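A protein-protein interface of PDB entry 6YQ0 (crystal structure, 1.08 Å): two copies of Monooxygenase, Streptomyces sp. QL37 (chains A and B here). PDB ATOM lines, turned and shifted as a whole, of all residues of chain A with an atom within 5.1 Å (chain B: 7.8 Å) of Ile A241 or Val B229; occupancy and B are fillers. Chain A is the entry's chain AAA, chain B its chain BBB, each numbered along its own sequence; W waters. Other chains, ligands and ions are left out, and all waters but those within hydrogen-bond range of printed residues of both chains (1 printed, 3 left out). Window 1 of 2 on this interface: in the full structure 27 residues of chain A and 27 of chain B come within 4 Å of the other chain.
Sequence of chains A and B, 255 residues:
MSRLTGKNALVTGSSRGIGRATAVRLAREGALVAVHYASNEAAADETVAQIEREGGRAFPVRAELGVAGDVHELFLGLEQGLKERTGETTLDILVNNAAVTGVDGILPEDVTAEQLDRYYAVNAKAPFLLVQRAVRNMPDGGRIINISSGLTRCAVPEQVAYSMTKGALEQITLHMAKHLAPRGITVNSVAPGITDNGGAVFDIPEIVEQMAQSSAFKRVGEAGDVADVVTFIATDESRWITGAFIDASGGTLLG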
ATOM      1  N   THR A 186       8.720 -16.112  20.964  1.00  0.00           N
ATOM      2  CA  THR A 186       9.294 -17.107  20.043  1.00  0.00           C
ATOM      3  C   THR A 186      10.767 -16.822  19.858  1.00  0.00           C
ATOM      4  O   THR A 186      11.228 -15.678  19.958  1.00  0.00           O
ATOM      5  CB  THR A 186       8.570 -17.198  18.728  1.00  0.00           C
ATOM      6  OG1 THR A 186       8.851 -16.002  17.962  1.00  0.00           O
ATOM      7  CG2 THR A 186       7.077 -17.400  18.883  1.00  0.00           C
ATOM      8  N   ASN A 188      13.861 -18.100  17.130  1.00  0.00           N
ATOM      9  CA  ASN A 188      14.096 -18.829  15.889  1.00  0.00           C
ATOM     10  C   ASN A 188      15.457 -18.456  15.324  1.00  0.00           C
ATOM     11  O   ASN A 188      15.950 -17.331  15.590  1.00  0.00           O
ATOM     12  CB  ASN A 188      13.036 -18.506  14.867  1.00  0.00           C
ATOM     13  CG  ASN A 188      11.702 -19.075  15.264  1.00  0.00           C
ATOM     14  OD1 ASN A 188      11.544 -20.310  15.298  1.00  0.00           O
ATOM     15  ND2 ASN A 188      10.717 -18.229  15.479  1.00  0.00           N
ATOM     16  N   PHE A 232       9.236 -11.165   8.322  1.00  0.00           N
ATOM     17  CA  PHE A 232       8.070 -12.004   8.560  1.00  0.00           C
ATOM     18  C   PHE A 232       8.123 -12.637   9.960  1.00  0.00           C
ATOM     19  O   PHE A 232       7.130 -12.673  10.687  1.00  0.00           O
ATOM     20  CB  PHE A 232       7.971 -13.111   7.510  1.00  0.00           C
ATOM     21  CG  PHE A 232       6.972 -14.170   7.886  1.00  0.00           C
ATOM     22  CD1 PHE A 232       5.624 -13.894   7.929  1.00  0.00           C
ATOM     23  CD2 PHE A 232       7.428 -15.417   8.320  1.00  0.00           C
ATOM     24  CE1 PHE A 232       4.720 -14.850   8.404  1.00  0.00           C
ATOM     25  CE2 PHE A 232       6.500 -16.358   8.797  1.00  0.00           C
ATOM     26  CZ  PHE A 232       5.178 -16.071   8.776  1.00  0.00           C
ATOM     27  N   ILE A 233       9.284 -13.186  10.325  1.00  0.00           N
ATOM     28  CA  ILE A 233       9.380 -13.840  11.646  1.00  0.00           C
ATOM     29  C   ILE A 233       9.057 -12.854  12.729  1.00  0.00           C
ATOM     30  O   ILE A 233       8.424 -13.198  13.762  1.00  0.00           O
ATOM     31  CB  ILE A 233      10.756 -14.519  11.844  1.00  0.00           C
ATOM     32  CG1 ILE A 233      10.959 -15.631  10.809  1.00  0.00           C
ATOM     33  CG2 ILE A 233      10.883 -15.034  13.270  1.00  0.00           C
ATOM     34  CD1 ILE A 233      10.049 -16.821  10.938  1.00  0.00           C
ATOM     35  N   GLU A 237       2.126 -13.136  12.501  1.00  0.00           N
ATOM     36  CA  GLU A 237       1.743 -14.311  11.717  1.00  0.00           C
ATOM     37  C   GLU A 237       2.742 -15.462  11.787  1.00  0.00           C
ATOM     38  O   GLU A 237       2.411 -16.560  11.318  1.00  0.00           O
ATOM     39  CB  GLU A 237       1.450 -13.952  10.279  1.00  0.00           C
ATOM     40  CG  GLU A 237       0.113 -13.260  10.052  1.00  0.00           C
ATOM     41  CD  GLU A 237       0.061 -11.874  10.667  1.00  0.00           C
ATOM     42  OE1 GLU A 237       1.000 -11.108  10.562  1.00  0.00           O
ATOM     43  OE2 GLU A 237      -1.033 -11.508  11.240  1.00  0.00           O
ATOM     44  N   SER A 238       3.887 -15.258  12.414  1.00  0.00           N
ATOM     45  CA  SER A 238       4.848 -16.325  12.670  1.00  0.00           C
ATOM     46  C   SER A 238       4.643 -16.975  14.038  1.00  0.00           C
ATOM     47  O   SER A 238       5.503 -17.759  14.440  1.00  0.00           O
ATOM     48  CB  SER A 238       6.243 -15.807  12.584  1.00  0.00           C
ATOM     49  OG  SER A 238       6.497 -15.029  13.766  1.00  0.00           O
ATOM     50  N   ARG A 239       3.562 -16.661  14.746  1.00  0.00           N
ATOM     51  CA  ARG A 239       3.419 -17.053  16.161  1.00  0.00           C
ATOM     52  C   ARG A 239       3.573 -18.529  16.398  1.00  0.00           C
ATOM     53  O   ARG A 239       3.934 -18.927  17.510  1.00  0.00           O
ATOM     54  CB  ARG A 239       2.092 -16.567  16.736  1.00  0.00           C
ATOM     55  CG  ARG A 239       0.875 -17.337  16.229  1.00  0.00           C
ATOM     56  CD  ARG A 239      -0.448 -16.678  16.542  1.00  0.00           C
ATOM     57  NE  ARG A 239      -0.765 -15.601  15.643  1.00  0.00           N
ATOM     58  CZ  ARG A 239      -1.224 -15.776  14.405  1.00  0.00           C
ATOM     59  NH1 ARG A 239      -1.526 -16.988  13.956  1.00  0.00           N
ATOM     60  NH2 ARG A 239      -1.381 -14.762  13.604  1.00  0.00           N
ATOM     61  N   TRP A 240       3.245 -19.355  15.422  1.00  0.00           N
ATOM     62  CA  TRP A 240       3.261 -20.804  15.577  1.00  0.00           C
ATOM     63  C   TRP A 240       4.595 -21.410  15.170  1.00  0.00           C
ATOM     64  O   TRP A 240       4.718 -22.673  15.190  1.00  0.00           O
ATOM     65  CB  TRP A 240       2.044 -21.405  14.875  1.00  0.00           C
ATOM     66  CG  TRP A 240       1.478 -22.612  15.499  1.00  0.00           C
ATOM     67  CD1 TRP A 240       1.217 -23.776  14.836  1.00  0.00           C
ATOM     68  CD2 TRP A 240       1.095 -22.778  16.847  1.00  0.00           C
ATOM     69  NE1 TRP A 240       0.720 -24.683  15.698  1.00  0.00           N
ATOM     70  CE2 TRP A 240       0.611 -24.141  16.921  1.00  0.00           C
ATOM     71  CE3 TRP A 240       1.047 -21.983  17.977  1.00  0.00           C
ATOM     72  CZ2 TRP A 240       0.174 -24.681  18.147  1.00  0.00           C
ATOM     73  CZ3 TRP A 240       0.611 -22.553  19.180  1.00  0.00           C
ATOM     74  CH2 TRP A 240       0.183 -23.889  19.233  1.00  0.00           C
ATOM     75  N   ILE A 241       5.579 -20.584  14.880  1.00  0.00           N
ATOM     76  CA  ILE A 241       6.962 -21.011  14.567  1.00  0.00           C
ATOM     77  C   ILE A 241       7.825 -20.655  15.776  1.00  0.00           C
ATOM     78  O   ILE A 241       8.042 -19.464  16.043  1.00  0.00           O
ATOM     79  CB  ILE A 241       7.494 -20.320  13.329  1.00  0.00           C
ATOM     80  CG1 ILE A 241       6.555 -20.518  12.123  1.00  0.00           C
ATOM     81  CG2 ILE A 241       8.888 -20.841  13.043  1.00  0.00           C
ATOM     82  CD1 ILE A 241       7.025 -19.742  10.895  1.00  0.00           C
ATOM     83  N   THR A 242       8.376 -21.641  16.483  1.00  0.00           N
ATOM     84  CA  THR A 242       9.380 -21.375  17.507  1.00  0.00           C
ATOM     85  C   THR A 242      10.356 -22.512  17.552  1.00  0.00           C
ATOM     86  O   THR A 242      10.014 -23.671  17.257  1.00  0.00           O
ATOM     87  CB  THR A 242       8.745 -21.093  18.857  1.00  0.00           C
ATOM     88  OG1 THR A 242       9.749 -20.433  19.652  1.00  0.00           O
ATOM     89  CG2 THR A 242       8.257 -22.333  19.592  1.00  0.00           C
ATOM     90  N   GLY A 243      11.574 -22.197  17.973  1.00  0.00           N
ATOM     91  CA  GLY A 243      12.635 -23.179  18.037  1.00  0.00           C
ATOM     92  C   GLY A 243      13.118 -23.661  16.716  1.00  0.00           C
ATOM     93  O   GLY A 243      13.774 -24.738  16.667  1.00  0.00           O
ATOM     94  N   ALA A 244      12.854 -22.968  15.656  1.00  0.00           N
ATOM     95  CA  ALA A 244      13.023 -23.456  14.283  1.00  0.00           C
ATOM     96  C   ALA A 244      14.298 -22.953  13.644  1.00  0.00           C
ATOM     97  O   ALA A 244      14.798 -21.869  13.979  1.00  0.00           O
ATOM     98  CB  ALA A 244      11.840 -23.084  13.430  1.00  0.00           C
ATOM     99  N   ILE A 246      15.198 -21.680  10.094  1.00  0.00           N
ATOM    100  CA  ILE A 246      14.540 -21.146   8.898  1.00  0.00           C
ATOM    101  C   ILE A 246      15.636 -20.917   7.854  1.00  0.00           C
ATOM    102  O   ILE A 246      16.488 -20.017   7.991  1.00  0.00           O
ATOM    103  CB  ILE A 246      13.767 -19.853   9.214  1.00  0.00           C
ATOM    104  CG1 ILE A 246      12.735 -20.073  10.317  1.00  0.00           C
ATOM    105  CG2 ILE A 246      13.156 -19.338   7.922  1.00  0.00           C
ATOM    106  CD1 ILE A 246      11.629 -21.019  10.025  1.00  0.00           C
ATOM    107  N   THR B  22      -6.485 -21.797   4.912  1.00  0.00           N
ATOM    108  CA  THR B  22      -5.489 -21.392   3.910  1.00  0.00           C
ATOM    109  C   THR B  22      -6.165 -20.712   2.708  1.00  0.00           C
ATOM    110  O   THR B  22      -5.759 -19.637   2.302  1.00  0.00           O
ATOM    111  CB  THR B  22      -4.660 -22.599   3.480  1.00  0.00           C
ATOM    112  OG1 THR B  22      -3.970 -23.128   4.615  1.00  0.00           O
ATOM    113  CG2 THR B  22      -3.617 -22.219   2.474  1.00  0.00           C
ATOM    114  N   ARG B  25      -7.270 -17.254   3.655  1.00  0.00           N
ATOM    115  CA  ARG B  25      -6.193 -16.278   3.773  1.00  0.00           C
ATOM    116  C   ARG B  25      -5.582 -15.939   2.417  1.00  0.00           C
ATOM    117  O   ARG B  25      -5.267 -14.760   2.164  1.00  0.00           O
ATOM    118  CB  ARG B  25      -5.136 -16.774   4.763  1.00  0.00           C
ATOM    119  CG  ARG B  25      -5.603 -16.547   6.183  1.00  0.00           C
ATOM    120  CD  ARG B  25      -4.954 -17.559   7.093  1.00  0.00           C
ATOM    121  NE  ARG B  25      -5.372 -17.379   8.472  1.00  0.00           N
ATOM    122  CZ  ARG B  25      -6.561 -17.626   8.946  1.00  0.00           C
ATOM    123  NH1 ARG B  25      -7.492 -18.236   8.222  1.00  0.00           N
ATOM    124  NH2 ARG B  25      -6.823 -17.268  10.209  1.00  0.00           N
ATOM    125  N   ILE B 145       3.664 -25.751  -2.159  1.00  0.00           N
ATOM    126  CA  ILE B 145       3.726 -25.847  -0.714  1.00  0.00           C
ATOM    127  C   ILE B 145       3.127 -27.183  -0.339  1.00  0.00           C
ATOM    128  O   ILE B 145       1.939 -27.441  -0.587  1.00  0.00           O
ATOM    129  CB  ILE B 145       3.027 -24.673   0.012  1.00  0.00           C
ATOM    130  CG1 ILE B 145       3.485 -23.339  -0.573  1.00  0.00           C
ATOM    131  CG2 ILE B 145       3.274 -24.778   1.479  1.00  0.00           C
ATOM    132  CD1 ILE B 145       2.716 -22.134  -0.150  1.00  0.00           C
ATOM    133  N   ILE B 147       2.020 -29.723   2.624  1.00  0.00           N
ATOM    134  CA  ILE B 147       1.692 -29.744   4.057  1.00  0.00           C
ATOM    135  C   ILE B 147       2.067 -31.114   4.588  1.00  0.00           C
ATOM    136  O   ILE B 147       1.448 -32.124   4.222  1.00  0.00           O
ATOM    137  CB  ILE B 147       0.217 -29.430   4.316  1.00  0.00           C
ATOM    138  CG1 ILE B 147      -0.259 -28.170   3.607  1.00  0.00           C
ATOM    139  CG2 ILE B 147      -0.016 -29.350   5.822  1.00  0.00           C
ATOM    140  CD1 ILE B 147       0.555 -26.918   3.928  1.00  0.00           C
ATOM    141  N   SER B 189       8.087 -27.496   2.444  1.00  0.00           N
ATOM    142  CA  SER B 189       7.211 -28.223   3.339  1.00  0.00           C
ATOM    143  C   SER B 189       6.817 -27.364   4.519  1.00  0.00           C
ATOM    144  O   SER B 189       7.705 -26.683   5.095  1.00  0.00           O
ATOM    145  CB  SER B 189       7.890 -29.443   3.906  1.00  0.00           C
ATOM    146  OG  SER B 189       8.316 -30.359   2.898  1.00  0.00           O
ATOM    147  N   VAL B 190       5.560 -27.377   4.914  1.00  0.00           N
ATOM    148  CA  VAL B 190       5.088 -26.748   6.154  1.00  0.00           C
ATOM    149  C   VAL B 190       4.562 -27.859   7.029  1.00  0.00           C
ATOM    150  O   VAL B 190       3.669 -28.598   6.578  1.00  0.00           O
ATOM    151  CB  VAL B 190       4.061 -25.643   5.890  1.00  0.00           C
ATOM    152  CG1 VAL B 190       3.493 -25.126   7.200  1.00  0.00           C
ATOM    153  CG2 VAL B 190       4.645 -24.532   5.046  1.00  0.00           C
ATOM    154  N   ALA B 191       5.088 -27.999   8.229  1.00  0.00           N
ATOM    155  CA  ALA B 191       4.777 -29.127   9.099  1.00  0.00           C
ATOM    156  C   ALA B 191       3.978 -28.684  10.309  1.00  0.00           C
ATOM    157  O   ALA B 191       4.544 -28.122  11.259  1.00  0.00           O
ATOM    158  CB  ALA B 191       6.077 -29.746   9.564  1.00  0.00           C
ATOM    159  N   PHE B 217       3.670 -24.202  23.759  1.00  0.00           N
ATOM    160  CA  PHE B 217       2.710 -23.176  24.190  1.00  0.00           C
ATOM    161  C   PHE B 217       1.548 -23.777  24.950  1.00  0.00           C
ATOM    162  O   PHE B 217       0.716 -23.015  25.429  1.00  0.00           O
ATOM    163  CB  PHE B 217       2.246 -22.353  22.977  1.00  0.00           C
ATOM    164  CG  PHE B 217       3.384 -21.699  22.259  1.00  0.00           C
ATOM    165  CD1 PHE B 217       4.179 -20.789  22.896  1.00  0.00           C
ATOM    166  CD2 PHE B 217       3.665 -21.992  20.945  1.00  0.00           C
ATOM    167  CE1 PHE B 217       5.223 -20.167  22.251  1.00  0.00           C
ATOM    168  CE2 PHE B 217       4.738 -21.350  20.294  1.00  0.00           C
ATOM    169  CZ  PHE B 217       5.452 -20.417  20.933  1.00  0.00           C
ATOM    170  N   ALA B 223      -6.347 -23.749  13.032  1.00  0.00           N
ATOM    171  CA  ALA B 223      -6.118 -23.834  11.599  1.00  0.00           C
ATOM    172  C   ALA B 223      -5.418 -22.589  11.088  1.00  0.00           C
ATOM    173  O   ALA B 223      -4.511 -22.701  10.226  1.00  0.00           O
ATOM    174  CB  ALA B 223      -7.412 -24.087  10.880  1.00  0.00           C
ATOM    175  N   GLY B 224      -5.798 -21.410  11.583  1.00  0.00           N
ATOM    176  CA  GLY B 224      -5.209 -20.187  11.089  1.00  0.00           C
ATOM    177  C   GLY B 224      -3.756 -20.060  11.486  1.00  0.00           C
ATOM    178  O   GLY B 224      -3.005 -19.349  10.789  1.00  0.00           O
ATOM    179  N   ASP B 225      -3.299 -20.665  12.583  1.00  0.00           N
ATOM    180  CA  ASP B 225      -1.867 -20.628  12.941  1.00  0.00           C
ATOM    181  C   ASP B 225      -1.027 -21.208  11.837  1.00  0.00           C
ATOM    182  O   ASP B 225       0.095 -20.710  11.550  1.00  0.00           O
ATOM    183  CB  ASP B 225      -1.637 -21.370  14.225  1.00  0.00           C
ATOM    184  CG  ASP B 225      -2.166 -20.726  15.471  1.00  0.00           C
ATOM    185  OD1 ASP B 225      -1.998 -19.486  15.623  1.00  0.00           O
ATOM    186  OD2 ASP B 225      -2.771 -21.428  16.300  1.00  0.00           O
ATOM    187  N   VAL B 226      -1.423 -22.336  11.289  1.00  0.00           N
ATOM    188  CA  VAL B 226      -0.737 -22.992  10.181  1.00  0.00           C
ATOM    189  C   VAL B 226      -0.957 -22.248   8.901  1.00  0.00           C
ATOM    190  O   VAL B 226       0.007 -21.989   8.126  1.00  0.00           O
ATOM    191  CB  VAL B 226      -1.160 -24.453  10.094  1.00  0.00           C
ATOM    192  CG1 VAL B 226      -0.517 -25.141   8.898  1.00  0.00           C
ATOM    193  CG2 VAL B 226      -0.917 -25.213  11.367  1.00  0.00           C
ATOM    194  N   ALA B 227      -2.201 -21.868   8.627  1.00  0.00           N
ATOM    195  CA  ALA B 227      -2.537 -21.190   7.370  1.00  0.00           C
ATOM    196  C   ALA B 227      -1.787 -19.870   7.233  1.00  0.00           C
ATOM    197  O   ALA B 227      -1.467 -19.473   6.126  1.00  0.00           O
ATOM    198  CB  ALA B 227      -4.031 -21.020   7.288  1.00  0.00           C
ATOM    199  N   ASP B 228      -1.531 -19.167   8.344  1.00  0.00           N
ATOM    200  CA  ASP B 228      -0.778 -17.901   8.255  1.00  0.00           C
ATOM    201  C   ASP B 228       0.625 -18.168   7.754  1.00  0.00           C
ATOM    202  O   ASP B 228       1.203 -17.330   7.006  1.00  0.00           O
ATOM    203  CB  ASP B 228      -0.736 -17.211   9.624  1.00  0.00           C
ATOM    204  CG  ASP B 228      -2.039 -16.535  10.013  1.00  0.00           C
ATOM    205  OD1 ASP B 228      -2.833 -16.181   9.109  1.00  0.00           O
ATOM    206  OD2 ASP B 228      -2.201 -16.271  11.243  1.00  0.00           O
ATOM    207  N   VAL B 229       1.243 -19.270   8.142  1.00  0.00           N
ATOM    208  CA  VAL B 229       2.598 -19.612   7.649  1.00  0.00           C
ATOM    209  C   VAL B 229       2.548 -19.998   6.179  1.00  0.00           C
ATOM    210  O   VAL B 229       3.347 -19.508   5.378  1.00  0.00           O
ATOM    211  CB  VAL B 229       3.180 -20.733   8.496  1.00  0.00           C
ATOM    212  CG1 VAL B 229       4.566 -21.120   7.944  1.00  0.00           C
ATOM    213  CG2 VAL B 229       3.307 -20.305   9.954  1.00  0.00           C
ATOM    214  N   VAL B 230       1.577 -20.812   5.801  1.00  0.00           N
ATOM    215  CA  VAL B 230       1.400 -21.185   4.384  1.00  0.00           C
ATOM    216  C   VAL B 230       1.253 -19.951   3.509  1.00  0.00           C
ATOM    217  O   VAL B 230       1.830 -19.817   2.447  1.00  0.00           O
ATOM    218  CB  VAL B 230       0.218 -22.146   4.210  1.00  0.00           C
ATOM    219  CG1 VAL B 230      -0.024 -22.438   2.724  1.00  0.00           C
ATOM    220  CG2 VAL B 230       0.431 -23.427   4.961  1.00  0.00           C
ATOM    221  N   THR B 231       0.430 -18.993   3.985  1.00  0.00           N
ATOM    222  CA  THR B 231       0.151 -17.758   3.250  1.00  0.00           C
ATOM    223  C   THR B 231       1.443 -16.998   3.039  1.00  0.00           C
ATOM    224  O   THR B 231       1.701 -16.499   1.932  1.00  0.00           O
ATOM    225  CB  THR B 231      -0.923 -16.946   3.972  1.00  0.00           C
ATOM    226  OG1 THR B 231      -2.140 -17.708   3.976  1.00  0.00           O
ATOM    227  CG2 THR B 231      -1.208 -15.639   3.262  1.00  0.00           C
ATOM    228  N   PHE B 232       2.258 -16.805   4.079  1.00  0.00           N
ATOM    229  CA  PHE B 232       3.544 -16.129   3.888  1.00  0.00           C
ATOM    230  C   PHE B 232       4.381 -16.856   2.826  1.00  0.00           C
ATOM    231  O   PHE B 232       4.965 -16.214   1.940  1.00  0.00           O
ATOM    232  CB  PHE B 232       4.331 -16.082   5.199  1.00  0.00           C
ATOM    233  CG  PHE B 232       5.764 -15.683   4.967  1.00  0.00           C
ATOM    234  CD1 PHE B 232       6.084 -14.404   4.562  1.00  0.00           C
ATOM    235  CD2 PHE B 232       6.774 -16.611   5.066  1.00  0.00           C
ATOM    236  CE1 PHE B 232       7.387 -14.082   4.253  1.00  0.00           C
ATOM    237  CE2 PHE B 232       8.085 -16.274   4.732  1.00  0.00           C
ATOM    238  CZ  PHE B 232       8.363 -15.024   4.344  1.00  0.00           C
ATOM    239  N   ILE B 233       4.464 -18.182   2.899  1.00  0.00           N
ATOM    240  CA  ILE B 233       5.286 -18.903   1.905  1.00  0.00           C
ATOM    241  C   ILE B 233       4.782 -18.595   0.490  1.00  0.00           C
ATOM    242  O   ILE B 233       5.552 -18.493  -0.457  1.00  0.00           O
ATOM    243  CB  ILE B 233       5.370 -20.391   2.235  1.00  0.00           C
ATOM    244  CG1 ILE B 233       6.086 -20.602   3.567  1.00  0.00           C
ATOM    245  CG2 ILE B 233       6.089 -21.149   1.101  1.00  0.00           C
ATOM    246  CD1 ILE B 233       7.520 -20.262   3.662  1.00  0.00           C
ATOM    247  N   ALA B 234       3.467 -18.489   0.315  1.00  0.00           N
ATOM    248  CA  ALA B 234       2.897 -18.191  -1.011  1.00  0.00           C
ATOM    249  C   ALA B 234       3.247 -16.815  -1.570  1.00  0.00           C
ATOM    250  O   ALA B 234       3.017 -16.614  -2.754  1.00  0.00           O
ATOM    251  CB  ALA B 234       1.379 -18.338  -0.932  1.00  0.00           C
ATOM    252  N   THR B 235       3.735 -15.892  -0.729  1.00  0.00           N
ATOM    253  CA  THR B 235       4.014 -14.518  -1.166  1.00  0.00           C
ATOM    254  C   THR B 235       5.405 -14.357  -1.738  1.00  0.00           C
ATOM    255  O   THR B 235       6.302 -15.219  -1.601  1.00  0.00           O
ATOM    256  CB  THR B 235       3.807 -13.518  -0.006  1.00  0.00           C
ATOM    257  OG1 THR B 235       4.836 -13.642   0.978  1.00  0.00           O
ATOM    258  CG2 THR B 235       2.416 -13.608   0.610  1.00  0.00           C
ATOM    259  N   SER B 238       8.928 -14.695   0.467  1.00  0.00           N
ATOM    260  CA  SER B 238       9.544 -15.970   0.780  1.00  0.00           C
ATOM    261  C   SER B 238      10.480 -16.444  -0.337  1.00  0.00           C
ATOM    262  O   SER B 238      10.933 -17.609  -0.278  1.00  0.00           O
ATOM    263  CB  SER B 238       8.505 -17.038   0.992  1.00  0.00           C
ATOM    264  OG  SER B 238       7.950 -17.373  -0.280  1.00  0.00           O
ATOM    265  N   ILE B 246       9.602 -26.155   7.127  1.00  0.00           N
ATOM    266  CA  ILE B 246       9.137 -25.013   7.937  1.00  0.00           C
ATOM    267  C   ILE B 246       8.283 -25.581   9.069  1.00  0.00           C
ATOM    268  O   ILE B 246       7.179 -26.109   8.807  1.00  0.00           O
ATOM    269  CB  ILE B 246       8.393 -23.993   7.081  1.00  0.00           C
ATOM    270  CG1 ILE B 246       9.246 -23.488   5.925  1.00  0.00           C
ATOM    271  CG2 ILE B 246       7.943 -22.854   7.978  1.00  0.00           C
ATOM    272  CD1 ILE B 246      10.455 -22.749   6.275  1.00  0.00           C
ATOM    273  N   ASP B 247       8.779 -25.428  10.292  1.00  0.00           N
ATOM    274  CA  ASP B 247       8.086 -25.955  11.462  1.00  0.00           C
ATOM    275  C   ASP B 247       6.912 -25.020  11.830  1.00  0.00           C
ATOM    276  O   ASP B 247       7.202 -23.867  12.277  1.00  0.00           O
ATOM    277  CB  ASP B 247       9.096 -26.092  12.593  1.00  0.00           C
ATOM    278  CG  ASP B 247       8.533 -26.691  13.837  1.00  0.00           C
ATOM    279  OD1 ASP B 247       7.362 -26.443  14.174  1.00  0.00           O
ATOM    280  OD2 ASP B 247       9.408 -27.279  14.614  1.00  0.00           O
ATOM    281  N   ALA B 248       5.734 -25.440  11.661  1.00  0.00           N
ATOM    282  CA  ALA B 248       4.547 -24.671  12.044  1.00  0.00           C
ATOM    283  C   ALA B 248       3.737 -25.489  13.058  1.00  0.00           C
ATOM    284  O   ALA B 248       2.542 -25.734  12.892  1.00  0.00           O
ATOM    285  CB  ALA B 248       3.714 -24.241  10.868  1.00  0.00           C
ATOM    286  N   SER B 249       4.415 -25.890  14.126  1.00  0.00           N
ATOM    287  CA  SER B 249       3.880 -26.860  15.111  1.00  0.00           C
ATOM    288  C   SER B 249       3.697 -26.243  16.465  1.00  0.00           C
ATOM    289  O   SER B 249       3.369 -27.000  17.425  1.00  0.00           O
ATOM    290  CB  SER B 249       4.701 -28.096  15.206  1.00  0.00           C
ATOM    291  OG  SER B 249       5.908 -27.879  15.930  1.00  0.00           O
ATOM    292  N   GLY B 250       3.926 -24.992  16.645  1.00  0.00           N
ATOM    293  CA  GLY B 250       3.846 -24.440  18.009  1.00  0.00           C
ATOM    294  C   GLY B 250       4.884 -25.038  18.913  1.00  0.00           C
ATOM    295  O   GLY B 250       4.590 -25.315  20.134  1.00  0.00           O
ATOM    296  N   GLY B 251       6.076 -25.284  18.443  1.00  0.00           N
ATOM    297  CA  GLY B 251       7.106 -25.816  19.335  1.00  0.00           C
ATOM    298  C   GLY B 251       6.873 -27.237  19.743  1.00  0.00           C
ATOM    299  O   GLY B 251       7.354 -27.636  20.833  1.00  0.00           O
HETATM  300  O   HOH W   1       1.818 -18.800  12.895  1.00  0.00           O
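N of Gly B250 is in hydrogen-bond range of O of Trp A240, at 2.8 Å.
The backbone NH of Ser B249 sits at hydrogen-bond distance from the backbone carbonyl oxygen of Trp A240.
The side-chain carboxylate of Asp B225 is in salt-bridge range of the guanidinium group of Arg A239 (3.0 Å).
NH1 of Arg A239 lies within salt-bridge range of OD2 of Asp B228, 2.9 Å away.
The side-chain carboxylate of Asp B247 lies within hydrogen-bond range of the side-chain hydroxyl of Ser B249 (2.7 Å).
O of Ile A241 lies within hydrogen-bond range of ND2 of Asn A188 (3.0 Å).
The side-chain hydroxyl (OG1) of Thr B235 lies within hydrogen-bond range of the backbone carbonyl oxygen (O) of Phe B232 (2.7 Å).
O of Ala B191 is in hydrogen-bond range of N of Ala B248, 3.0 Å away.
The side-chain carboxylate of Asp B228 lies within salt-bridge range of the guanidinium group of Arg B25.
Among the printed residues, merely in contact across the chains: Trp A240 with Ala B248 (3.1 Å), Ile A241 with Asp B247 (3.4 Å), Phe A232 with Phe B232 (3.4 Å), Trp A240 with Phe B217 (3.6 Å), Trp A240 with Asp B225 (3.6 Å), Glu A237 with Asp B228 (3.6 Å), Thr A242 with Phe B217 (3.7 Å), Thr A242 with Gly B251 (3.7 Å), Arg A239 with Phe B217 (3.8 Å), Ile A241 with Val B229 (3.9 Å) and Thr A186 with Phe B217 (3.99 Å).
Of the printed residues of chain B, Phe A232 touches Phe B232.
Of chain B, only Val B229 (3.9 Å) and Asp B247 (3.4 Å) come within 4 Å of Ile A241.
Of the printed residues of chain A, Phe B217 touches Thr A186, Arg A239, Trp A240 and Thr A242.
Printed residues of chain A within 4 Å of Asp B225: Arg A239 (3.0 Å) and Trp A240 (3.6 Å).
Val B229 touches just one residue of chain A: Ile A241.
Printed residues of chain A within 4 Å of Phe B232: Phe A232.
Of the printed residues of chain A, Ala B248 touches Trp A240.
The nearest residue of chain A that does not touch Val B229 is Glu A237 (4.1 Å).
Of the 13 printed residues of chain A, 7 touch a printed residue of chain B.
Hydrophobic or aromatic side chains of chain A within 4 Å of the printed part of chain B: Phe A232, Trp A240 and Ile A241.
Of the 28 printed residues of chain B, 10 touch a printed residue of chain A.
Among the printed residues, 15 pairs touch across the chains.
Among the printed residues, Asp or Glu carboxylates within 4 Å of a Lys or Arg side-chain nitrogen of the other chain: Arg A239 with Asp B225 (3.0 Å) and Arg A239 with Asp B228 (2.9 Å).
Phe B232 touches its own counterpart, Phe A232.
Positions printed for both chains: 232, 233, 238 and 246.
Of the 15 pairs that touch across the chains among the printed residues, 1 has its exchanged pair printed and touching as well.
Water W1 lies within hydrogen-bond range of O of Glu A237 (2.8 Å), O of Asp B225 (2.9 Å), N of Trp A240 (3.0 Å) and N of Arg A239 (3.3 Å).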
